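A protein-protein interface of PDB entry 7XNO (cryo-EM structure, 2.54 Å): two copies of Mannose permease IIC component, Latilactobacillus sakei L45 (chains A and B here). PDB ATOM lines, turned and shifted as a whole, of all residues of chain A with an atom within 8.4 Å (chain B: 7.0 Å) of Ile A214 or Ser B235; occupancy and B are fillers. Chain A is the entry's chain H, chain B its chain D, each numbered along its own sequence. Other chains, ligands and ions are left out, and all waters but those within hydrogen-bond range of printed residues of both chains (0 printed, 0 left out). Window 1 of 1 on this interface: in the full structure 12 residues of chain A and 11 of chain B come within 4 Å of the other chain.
The side-chain hydroxyl of Ser B235 is in hydrogen-bond range of the backbone carbonyl oxygen of Pro A210.
O of Ala B231 sits at hydrogen-bond distance from OG of Ser B235.
OE2 of Glu A207 is in hydrogen-bond range of OH of Tyr A240.
Among the printed residues, pairs that only touch across the chains: Pro A210 with Leu B238 (3.8 Å), Pro A210 with Ile B239 (3.7 Å), Phe A211 with Ile B239 (3.95 Å), Ala A213 with Ser B235 (3.3 Å), Ile A214 with Ser B235 (3.6 Å), Ile A214 with Ile B239 (3.9 Å), Val A217 with Ala B231 (3.9 Å), Val A217 with Ile B232 (3.6 Å) and Tyr A240 with Ile B239 (3.998 Å).
Of the printed residues of chain B, Pro A210 touches Ser B235 (3.4 Å), Leu B238 (3.8 Å) and Ile B239 (3.7 Å).
Printed residues of chain B within 4 Å of Phe A211: Ile B239.
Printed residues of chain B within 4 Å of Ala A213: Ser B235 (3.3 Å).
Of chain B, only Ser B235 (3.6 Å) and Ile B239 (3.9 Å) come within 4 Å of Ile A214.
Gly B230 touches none of the printed residues of chain A.
Ser B235 touches just these residues of chain A: Pro A210 (3.4 Å), Ala A213 (3.3 Å) and Ile A214 (3.6 Å).
Of the printed residues of chain A, Leu B238 touches Pro A210 (3.8 Å).
Of the printed residues of chain A, Ile B239 touches Pro A210, Phe A211, Ile A214 and Tyr A240.
The nearest residue of chain A that does not touch Ser B235 is Phe A211 (5.2 Å).
The nearest printed residue of chain A that does not touch Ile B239 is Glu A207 (5.5 Å).
Of the 21 printed residues of chain A, 6 touch a printed residue of chain B.
Hydrophobic or aromatic side chains of chain B that line the printed part of chain A: Ala B231, Ile B232, Leu B238 and Ile B239.
Among the printed residues, no Asp or Glu carboxylate lies within 4 Å of a Lys or Arg side-chain nitrogen of the other chain.
5 positions are printed for both chains.
Of the 10 pairs that touch across the chains among the printed residues, none has its exchanged pair printed and touching as well.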
ATOM      1  N   GLU A 207      29.105   1.410  18.312  1.00  0.00           N
ATOM      2  CA  GLU A 207      27.980   0.723  17.697  1.00  0.00           C
ATOM      3  C   GLU A 207      27.595   1.312  16.343  1.00  0.00           C
ATOM      4  O   GLU A 207      26.911   0.642  15.561  1.00  0.00           O
ATOM      5  CB  GLU A 207      26.786   0.754  18.660  1.00  0.00           C
ATOM      6  CG  GLU A 207      25.526   0.059  18.181  1.00  0.00           C
ATOM      7  CD  GLU A 207      24.306   0.498  18.959  1.00  0.00           C
ATOM      8  OE1 GLU A 207      24.290   1.655  19.426  1.00  0.00           O
ATOM      9  OE2 GLU A 207      23.363  -0.307  19.102  1.00  0.00           O
ATOM     10  N   VAL A 208      28.041   2.530  16.034  1.00  0.00           N
ATOM     11  CA  VAL A 208      27.724   3.174  14.762  1.00  0.00           C
ATOM     12  C   VAL A 208      28.935   3.330  13.854  1.00  0.00           C
ATOM     13  O   VAL A 208      28.770   3.764  12.702  1.00  0.00           O
ATOM     14  CB  VAL A 208      27.048   4.545  14.975  1.00  0.00           C
ATOM     15  CG1 VAL A 208      25.636   4.365  15.506  1.00  0.00           C
ATOM     16  CG2 VAL A 208      27.873   5.404  15.912  1.00  0.00           C
ATOM     17  N   TRP A 209      30.138   3.007  14.327  1.00  0.00           N
ATOM     18  CA  TRP A 209      31.312   3.033  13.459  1.00  0.00           C
ATOM     19  C   TRP A 209      31.183   2.137  12.227  1.00  0.00           C
ATOM     20  O   TRP A 209      31.650   2.551  11.149  1.00  0.00           O
ATOM     21  CB  TRP A 209      32.563   2.661  14.267  1.00  0.00           C
ATOM     22  CG  TRP A 209      33.229   3.825  14.938  1.00  0.00           C
ATOM     23  CD1 TRP A 209      33.371   4.023  16.278  1.00  0.00           C
ATOM     24  CD2 TRP A 209      33.849   4.948  14.300  1.00  0.00           C
ATOM     25  NE1 TRP A 209      34.037   5.199  16.518  1.00  0.00           N
ATOM     26  CE2 TRP A 209      34.342   5.786  15.319  1.00  0.00           C
ATOM     27  CE3 TRP A 209      34.033   5.328  12.967  1.00  0.00           C
ATOM     28  CZ2 TRP A 209      35.008   6.979  15.047  1.00  0.00           C
ATOM     29  CZ3 TRP A 209      34.692   6.512  12.700  1.00  0.00           C
ATOM     30  CH2 TRP A 209      35.172   7.322  13.735  1.00  0.00           C
ATOM     31  N   PRO A 210      30.622   0.919  12.305  1.00  0.00           N
ATOM     32  CA  PRO A 210      30.457   0.126  11.075  1.00  0.00           C
ATOM     33  C   PRO A 210      29.680   0.842   9.985  1.00  0.00           C
ATOM     34  O   PRO A 210      29.997   0.681   8.802  1.00  0.00           O
ATOM     35  CB  PRO A 210      29.717  -1.123  11.570  1.00  0.00           C
ATOM     36  CG  PRO A 210      30.147  -1.273  12.967  1.00  0.00           C
ATOM     37  CD  PRO A 210      30.303   0.118  13.504  1.00  0.00           C
ATOM     38  N   PHE A 211      28.664   1.626  10.348  1.00  0.00           N
ATOM     39  CA  PHE A 211      27.925   2.380   9.340  1.00  0.00           C
ATOM     40  C   PHE A 211      28.804   3.448   8.700  1.00  0.00           C
ATOM     41  O   PHE A 211      28.711   3.693   7.491  1.00  0.00           O
ATOM     42  CB  PHE A 211      26.677   2.999   9.964  1.00  0.00           C
ATOM     43  CG  PHE A 211      25.729   1.987  10.537  1.00  0.00           C
ATOM     44  CD1 PHE A 211      24.852   1.298   9.716  1.00  0.00           C
ATOM     45  CD2 PHE A 211      25.726   1.713  11.893  1.00  0.00           C
ATOM     46  CE1 PHE A 211      23.984   0.362  10.241  1.00  0.00           C
ATOM     47  CE2 PHE A 211      24.861   0.778  12.423  1.00  0.00           C
ATOM     48  CZ  PHE A 211      23.989   0.102  11.595  1.00  0.00           C
ATOM     49  N   PHE A 212      29.666   4.085   9.494  1.00  0.00           N
ATOM     50  CA  PHE A 212      30.631   5.029   8.941  1.00  0.00           C
ATOM     51  C   PHE A 212      31.541   4.341   7.933  1.00  0.00           C
ATOM     52  O   PHE A 212      31.797   4.873   6.846  1.00  0.00           O
ATOM     53  CB  PHE A 212      31.451   5.655  10.073  1.00  0.00           C
ATOM     54  CG  PHE A 212      32.463   6.671   9.610  1.00  0.00           C
ATOM     55  CD1 PHE A 212      33.725   6.277   9.191  1.00  0.00           C
ATOM     56  CD2 PHE A 212      32.156   8.020   9.610  1.00  0.00           C
ATOM     57  CE1 PHE A 212      34.653   7.209   8.768  1.00  0.00           C
ATOM     58  CE2 PHE A 212      33.083   8.955   9.193  1.00  0.00           C
ATOM     59  CZ  PHE A 212      34.331   8.550   8.770  1.00  0.00           C
ATOM     60  N   ALA A 213      32.039   3.151   8.280  1.00  0.00           N
ATOM     61  CA  ALA A 213      32.921   2.428   7.368  1.00  0.00           C
ATOM     62  C   ALA A 213      32.194   2.031   6.087  1.00  0.00           C
ATOM     63  O   ALA A 213      32.748   2.146   4.987  1.00  0.00           O
ATOM     64  CB  ALA A 213      33.496   1.196   8.065  1.00  0.00           C
ATOM     65  N   ILE A 214      30.951   1.561   6.213  1.00  0.00           N
ATOM     66  CA  ILE A 214      30.182   1.163   5.036  1.00  0.00           C
ATOM     67  C   ILE A 214      29.938   2.360   4.128  1.00  0.00           C
ATOM     68  O   ILE A 214      30.075   2.263   2.904  1.00  0.00           O
ATOM     69  CB  ILE A 214      28.861   0.493   5.455  1.00  0.00           C
ATOM     70  CG1 ILE A 214      29.134  -0.848   6.131  1.00  0.00           C
ATOM     71  CG2 ILE A 214      27.958   0.291   4.250  1.00  0.00           C
ATOM     72  CD1 ILE A 214      27.893  -1.524   6.664  1.00  0.00           C
ATOM     73  N   GLY A 215      29.573   3.506   4.708  1.00  0.00           N
ATOM     74  CA  GLY A 215      29.382   4.699   3.900  1.00  0.00           C
ATOM     75  C   GLY A 215      30.658   5.155   3.221  1.00  0.00           C
ATOM     76  O   GLY A 215      30.648   5.532   2.046  1.00  0.00           O
ATOM     77  N   PHE A 216      31.779   5.110   3.948  1.00  0.00           N
ATOM     78  CA  PHE A 216      33.058   5.501   3.367  1.00  0.00           C
ATOM     79  C   PHE A 216      33.422   4.613   2.185  1.00  0.00           C
ATOM     80  O   PHE A 216      33.886   5.103   1.150  1.00  0.00           O
ATOM     81  CB  PHE A 216      34.150   5.451   4.438  1.00  0.00           C
ATOM     82  CG  PHE A 216      35.504   5.891   3.953  1.00  0.00           C
ATOM     83  CD1 PHE A 216      35.880   7.220   4.029  1.00  0.00           C
ATOM     84  CD2 PHE A 216      36.406   4.974   3.438  1.00  0.00           C
ATOM     85  CE1 PHE A 216      37.123   7.628   3.590  1.00  0.00           C
ATOM     86  CE2 PHE A 216      37.648   5.377   2.997  1.00  0.00           C
ATOM     87  CZ  PHE A 216      38.007   6.705   3.075  1.00  0.00           C
ATOM     88  N   VAL A 217      33.219   3.301   2.320  1.00  0.00           N
ATOM     89  CA  VAL A 217      33.565   2.396   1.228  1.00  0.00           C
ATOM     90  C   VAL A 217      32.605   2.568   0.055  1.00  0.00           C
ATOM     91  O   VAL A 217      33.024   2.574  -1.109  1.00  0.00           O
ATOM     92  CB  VAL A 217      33.602   0.940   1.724  1.00  0.00           C
ATOM     93  CG1 VAL A 217      33.837   0.000   0.559  1.00  0.00           C
ATOM     94  CG2 VAL A 217      34.688   0.767   2.771  1.00  0.00           C
ATOM     95  N   LEU A 218      31.308   2.715   0.334  1.00  0.00           N
ATOM     96  CA  LEU A 218      30.331   2.853  -0.738  1.00  0.00           C
ATOM     97  C   LEU A 218      30.449   4.183  -1.467  1.00  0.00           C
ATOM     98  O   LEU A 218      29.991   4.289  -2.609  1.00  0.00           O
ATOM     99  CB  LEU A 218      28.915   2.686  -0.187  1.00  0.00           C
ATOM    100  CG  LEU A 218      28.467   1.261   0.141  1.00  0.00           C
ATOM    101  CD1 LEU A 218      26.956   1.197   0.281  1.00  0.00           C
ATOM    102  CD2 LEU A 218      28.953   0.282  -0.914  1.00  0.00           C
ATOM    103  N   ALA A 219      31.040   5.199  -0.837  1.00  0.00           N
ATOM    104  CA  ALA A 219      31.254   6.461  -1.534  1.00  0.00           C
ATOM    105  C   ALA A 219      32.310   6.351  -2.625  1.00  0.00           C
ATOM    106  O   ALA A 219      32.360   7.211  -3.509  1.00  0.00           O
ATOM    107  CB  ALA A 219      31.648   7.552  -0.539  1.00  0.00           C
ATOM    108  N   THR A 220      33.154   5.317  -2.585  1.00  0.00           N
ATOM    109  CA  THR A 220      34.154   5.124  -3.629  1.00  0.00           C
ATOM    110  C   THR A 220      33.544   4.708  -4.959  1.00  0.00           C
ATOM    111  O   THR A 220      34.230   4.777  -5.984  1.00  0.00           O
ATOM    112  CB  THR A 220      35.186   4.083  -3.193  1.00  0.00           C
ATOM    113  OG1 THR A 220      34.516   2.894  -2.761  1.00  0.00           O
ATOM    114  CG2 THR A 220      36.035   4.621  -2.057  1.00  0.00           C
ATOM    115  N   ILE A 221      32.286   4.274  -4.970  1.00  0.00           N
ATOM    116  CA  ILE A 221      31.574   4.000  -6.213  1.00  0.00           C
ATOM    117  C   ILE A 221      31.097   5.337  -6.770  1.00  0.00           C
ATOM    118  O   ILE A 221      30.151   5.933  -6.251  1.00  0.00           O
ATOM    119  CB  ILE A 221      30.405   3.034  -5.995  1.00  0.00           C
ATOM    120  CG1 ILE A 221      30.893   1.752  -5.321  1.00  0.00           C
ATOM    121  CG2 ILE A 221      29.721   2.719  -7.314  1.00  0.00           C
ATOM    122  CD1 ILE A 221      29.819   1.017  -4.555  1.00  0.00           C
ATOM    123  N   LEU A 224      27.327   6.262  -7.710  1.00  0.00           N
ATOM    124  CA  LEU A 224      26.314   6.493  -6.689  1.00  0.00           C
ATOM    125  C   LEU A 224      26.285   7.970  -6.321  1.00  0.00           C
ATOM    126  O   LEU A 224      27.331   8.569  -6.058  1.00  0.00           O
ATOM    127  CB  LEU A 224      26.592   5.647  -5.447  1.00  0.00           C
ATOM    128  CG  LEU A 224      26.294   4.149  -5.519  1.00  0.00           C
ATOM    129  CD1 LEU A 224      26.720   3.462  -4.233  1.00  0.00           C
ATOM    130  CD2 LEU A 224      24.820   3.908  -5.789  1.00  0.00           C
ATOM    131  N   LEU A 229      23.126   7.539  -1.533  1.00  0.00           N
ATOM    132  CA  LEU A 229      23.818   7.185  -0.297  1.00  0.00           C
ATOM    133  C   LEU A 229      22.980   7.539   0.925  1.00  0.00           C
ATOM    134  O   LEU A 229      22.937   6.779   1.898  1.00  0.00           O
ATOM    135  CB  LEU A 229      25.179   7.880  -0.243  1.00  0.00           C
ATOM    136  CG  LEU A 229      26.241   7.344  -1.204  1.00  0.00           C
ATOM    137  CD1 LEU A 229      27.326   8.378  -1.450  1.00  0.00           C
ATOM    138  CD2 LEU A 229      26.840   6.049  -0.679  1.00  0.00           C
ATOM    139  N   ILE A 232      20.292   4.934   1.236  1.00  0.00           N
ATOM    140  CA  ILE A 232      20.867   3.710   1.786  1.00  0.00           C
ATOM    141  C   ILE A 232      21.062   3.843   3.290  1.00  0.00           C
ATOM    142  O   ILE A 232      20.751   2.923   4.056  1.00  0.00           O
ATOM    143  CB  ILE A 232      22.190   3.364   1.077  1.00  0.00           C
ATOM    144  CG1 ILE A 232      21.933   2.855  -0.339  1.00  0.00           C
ATOM    145  CG2 ILE A 232      22.962   2.320   1.866  1.00  0.00           C
ATOM    146  CD1 ILE A 232      23.199   2.486  -1.078  1.00  0.00           C
ATOM    147  N   GLY A 233      21.584   4.986   3.737  1.00  0.00           N
ATOM    148  CA  GLY A 233      21.780   5.191   5.163  1.00  0.00           C
ATOM    149  C   GLY A 233      20.480   5.194   5.941  1.00  0.00           C
ATOM    150  O   GLY A 233      20.393   4.613   7.027  1.00  0.00           O
ATOM    151  N   LEU A 236      19.224   1.619   6.134  1.00  0.00           N
ATOM    152  CA  LEU A 236      20.010   0.851   7.093  1.00  0.00           C
ATOM    153  C   LEU A 236      19.639   1.215   8.523  1.00  0.00           C
ATOM    154  O   LEU A 236      19.529   0.336   9.385  1.00  0.00           O
ATOM    155  CB  LEU A 236      21.501   1.075   6.851  1.00  0.00           C
ATOM    156  CG  LEU A 236      22.103   0.367   5.637  1.00  0.00           C
ATOM    157  CD1 LEU A 236      23.614   0.515   5.628  1.00  0.00           C
ATOM    158  CD2 LEU A 236      21.701  -1.097   5.620  1.00  0.00           C
ATOM    159  N   TYR A 240      18.069  -1.411  11.173  1.00  0.00           N
ATOM    160  CA  TYR A 240      18.728  -1.618  12.456  1.00  0.00           C
ATOM    161  C   TYR A 240      17.780  -1.343  13.615  1.00  0.00           C
ATOM    162  O   TYR A 240      17.735  -2.110  14.584  1.00  0.00           O
ATOM    163  CB  TYR A 240      19.966  -0.728  12.550  1.00  0.00           C
ATOM    164  CG  TYR A 240      20.921  -1.104  13.658  1.00  0.00           C
ATOM    165  CD1 TYR A 240      21.897  -2.068  13.458  1.00  0.00           C
ATOM    166  CD2 TYR A 240      20.848  -0.492  14.900  1.00  0.00           C
ATOM    167  CE1 TYR A 240      22.774  -2.413  14.466  1.00  0.00           C
ATOM    168  CE2 TYR A 240      21.720  -0.830  15.914  1.00  0.00           C
ATOM    169  CZ  TYR A 240      22.681  -1.792  15.691  1.00  0.00           C
ATOM    170  OH  TYR A 240      23.552  -2.135  16.698  1.00  0.00           O
ATOM    171  N   LEU B 229      36.269  -3.983   0.382  1.00  0.00           N
ATOM    172  CA  LEU B 229      35.461  -5.177   0.610  1.00  0.00           C
ATOM    173  C   LEU B 229      35.704  -5.751   2.000  1.00  0.00           C
ATOM    174  O   LEU B 229      34.764  -6.192   2.672  1.00  0.00           O
ATOM    175  CB  LEU B 229      35.759  -6.221  -0.466  1.00  0.00           C
ATOM    176  CG  LEU B 229      35.235  -5.906  -1.869  1.00  0.00           C
ATOM    177  CD1 LEU B 229      35.980  -6.711  -2.921  1.00  0.00           C
ATOM    178  CD2 LEU B 229      33.739  -6.158  -1.955  1.00  0.00           C
ATOM    179  N   GLY B 230      36.960  -5.757   2.448  1.00  0.00           N
ATOM    180  CA  GLY B 230      37.254  -6.232   3.790  1.00  0.00           C
ATOM    181  C   GLY B 230      36.632  -5.364   4.866  1.00  0.00           C
ATOM    182  O   GLY B 230      36.137  -5.870   5.874  1.00  0.00           O
ATOM    183  N   ALA B 231      36.652  -4.045   4.667  1.00  0.00           N
ATOM    184  CA  ALA B 231      36.005  -3.143   5.613  1.00  0.00           C
ATOM    185  C   ALA B 231      34.498  -3.364   5.642  1.00  0.00           C
ATOM    186  O   ALA B 231      33.881  -3.346   6.712  1.00  0.00           O
ATOM    187  CB  ALA B 231      36.332  -1.693   5.262  1.00  0.00           C
ATOM    188  N   ILE B 232      33.890  -3.580   4.472  1.00  0.00           N
ATOM    189  CA  ILE B 232      32.462  -3.884   4.423  1.00  0.00           C
ATOM    190  C   ILE B 232      32.167  -5.173   5.177  1.00  0.00           C
ATOM    191  O   ILE B 232      31.198  -5.255   5.941  1.00  0.00           O
ATOM    192  CB  ILE B 232      31.974  -3.962   2.964  1.00  0.00           C
ATOM    193  CG1 ILE B 232      31.895  -2.570   2.342  1.00  0.00           C
ATOM    194  CG2 ILE B 232      30.615  -4.636   2.890  1.00  0.00           C
ATOM    195  CD1 ILE B 232      31.406  -2.584   0.913  1.00  0.00           C
ATOM    196  N   GLY B 233      32.992  -6.200   4.972  1.00  0.00           N
ATOM    197  CA  GLY B 233      32.780  -7.457   5.672  1.00  0.00           C
ATOM    198  C   GLY B 233      32.928  -7.326   7.175  1.00  0.00           C
ATOM    199  O   GLY B 233      32.142  -7.894   7.938  1.00  0.00           O
ATOM    200  N   ILE B 234      33.935  -6.571   7.623  1.00  0.00           N
ATOM    201  CA  ILE B 234      34.133  -6.362   9.055  1.00  0.00           C
ATOM    202  C   ILE B 234      32.955  -5.604   9.652  1.00  0.00           C
ATOM    203  O   ILE B 234      32.465  -5.942  10.736  1.00  0.00           O
ATOM    204  CB  ILE B 234      35.466  -5.634   9.311  1.00  0.00           C
ATOM    205  CG1 ILE B 234      36.646  -6.542   8.964  1.00  0.00           C
ATOM    206  CG2 ILE B 234      35.562  -5.178  10.757  1.00  0.00           C
ATOM    207  CD1 ILE B 234      37.972  -5.824   8.927  1.00  0.00           C
ATOM    208  N   SER B 235      32.484  -4.566   8.957  1.00  0.00           N
ATOM    209  CA  SER B 235      31.338  -3.807   9.446  1.00  0.00           C
ATOM    210  C   SER B 235      30.086  -4.672   9.509  1.00  0.00           C
ATOM    211  O   SER B 235      29.309  -4.582  10.467  1.00  0.00           O
ATOM    212  CB  SER B 235      31.104  -2.587   8.557  1.00  0.00           C
ATOM    213  OG  SER B 235      32.299  -1.848   8.387  1.00  0.00           O
ATOM    214  N   LEU B 236      29.870  -5.513   8.495  1.00  0.00           N
ATOM    215  CA  LEU B 236      28.712  -6.400   8.503  1.00  0.00           C
ATOM    216  C   LEU B 236      28.796  -7.400   9.648  1.00  0.00           C
ATOM    217  O   LEU B 236      27.790  -7.680  10.310  1.00  0.00           O
ATOM    218  CB  LEU B 236      28.595  -7.124   7.163  1.00  0.00           C
ATOM    219  CG  LEU B 236      28.079  -6.291   5.990  1.00  0.00           C
ATOM    220  CD1 LEU B 236      27.816  -7.174   4.782  1.00  0.00           C
ATOM    221  CD2 LEU B 236      26.826  -5.530   6.386  1.00  0.00           C
ATOM    222  N   ALA B 237      29.987  -7.950   9.896  1.00  0.00           N
ATOM    223  CA  ALA B 237      30.158  -8.863  11.020  1.00  0.00           C
ATOM    224  C   ALA B 237      29.877  -8.164  12.345  1.00  0.00           C
ATOM    225  O   ALA B 237      29.218  -8.728  13.225  1.00  0.00           O
ATOM    226  CB  ALA B 237      31.569  -9.448  11.013  1.00  0.00           C
ATOM    227  N   LEU B 238      30.371  -6.933  12.503  1.00  0.00           N
ATOM    228  CA  LEU B 238      30.133  -6.191  13.737  1.00  0.00           C
ATOM    229  C   LEU B 238      28.649  -5.907  13.936  1.00  0.00           C
ATOM    230  O   LEU B 238      28.126  -6.054  15.046  1.00  0.00           O
ATOM    231  CB  LEU B 238      30.931  -4.888  13.728  1.00  0.00           C
ATOM    232  CG  LEU B 238      32.441  -5.009  13.943  1.00  0.00           C
ATOM    233  CD1 LEU B 238      33.133  -3.696  13.617  1.00  0.00           C
ATOM    234  CD2 LEU B 238      32.750  -5.441  15.365  1.00  0.00           C
ATOM    235  N   ILE B 239      27.955  -5.508  12.869  1.00  0.00           N
ATOM    236  CA  ILE B 239      26.527  -5.220  12.972  1.00  0.00           C
ATOM    237  C   ILE B 239      25.747  -6.487  13.301  1.00  0.00           C
ATOM    238  O   ILE B 239      24.829  -6.471  14.131  1.00  0.00           O
ATOM    239  CB  ILE B 239      26.025  -4.559  11.675  1.00  0.00           C
ATOM    240  CG1 ILE B 239      26.527  -3.117  11.583  1.00  0.00           C
ATOM    241  CG2 ILE B 239      24.508  -4.595  11.599  1.00  0.00           C
ATOM    242  CD1 ILE B 239      26.609  -2.589  10.168  1.00  0.00           C
ATOM    243  N   TYR B 240      26.099  -7.603  12.658  1.00  0.00           N
ATOM    244  CA  TYR B 240      25.424  -8.866  12.932  1.00  0.00           C
ATOM    245  C   TYR B 240      25.638  -9.301  14.375  1.00  0.00           C
ATOM    246  O   TYR B 240      24.697  -9.743  15.043  1.00  0.00           O
ATOM    247  CB  TYR B 240      25.921  -9.939  11.966  1.00  0.00           C
ATOM    248  CG  TYR B 240      25.053 -11.172  11.904  1.00  0.00           C
ATOM    249  CD1 TYR B 240      23.953 -11.225  11.061  1.00  0.00           C
ATOM    250  CD2 TYR B 240      25.335 -12.284  12.684  1.00  0.00           C
ATOM    251  CE1 TYR B 240      23.157 -12.350  10.998  1.00  0.00           C
ATOM    252  CE2 TYR B 240      24.544 -13.412  12.628  1.00  0.00           C
ATOM    253  CZ  TYR B 240      23.457 -13.441  11.784  1.00  0.00           C
ATOM    254  OH  TYR B 240      22.664 -14.563  11.724  1.00  0.00           O
ATOM    255  N   LEU B 241      26.868  -9.175  14.879  1.00  0.00           N
ATOM    256  CA  LEU B 241      27.131  -9.524  16.271  1.00  0.00           C
ATOM    257  C   LEU B 241      26.356  -8.623  17.223  1.00  0.00           C
ATOM    258  O   LEU B 241      25.795  -9.096  18.217  1.00  0.00           O
ATOM    259  CB  LEU B 241      28.630  -9.446  16.556  1.00  0.00           C
ATOM    260  CG  LEU B 241      29.484 -10.577  15.980  1.00  0.00           C
ATOM    261  CD1 LEU B 241      30.954 -10.345  16.283  1.00  0.00           C
ATOM    262  CD2 LEU B 241      29.032 -11.921  16.523  1.00  0.00           C
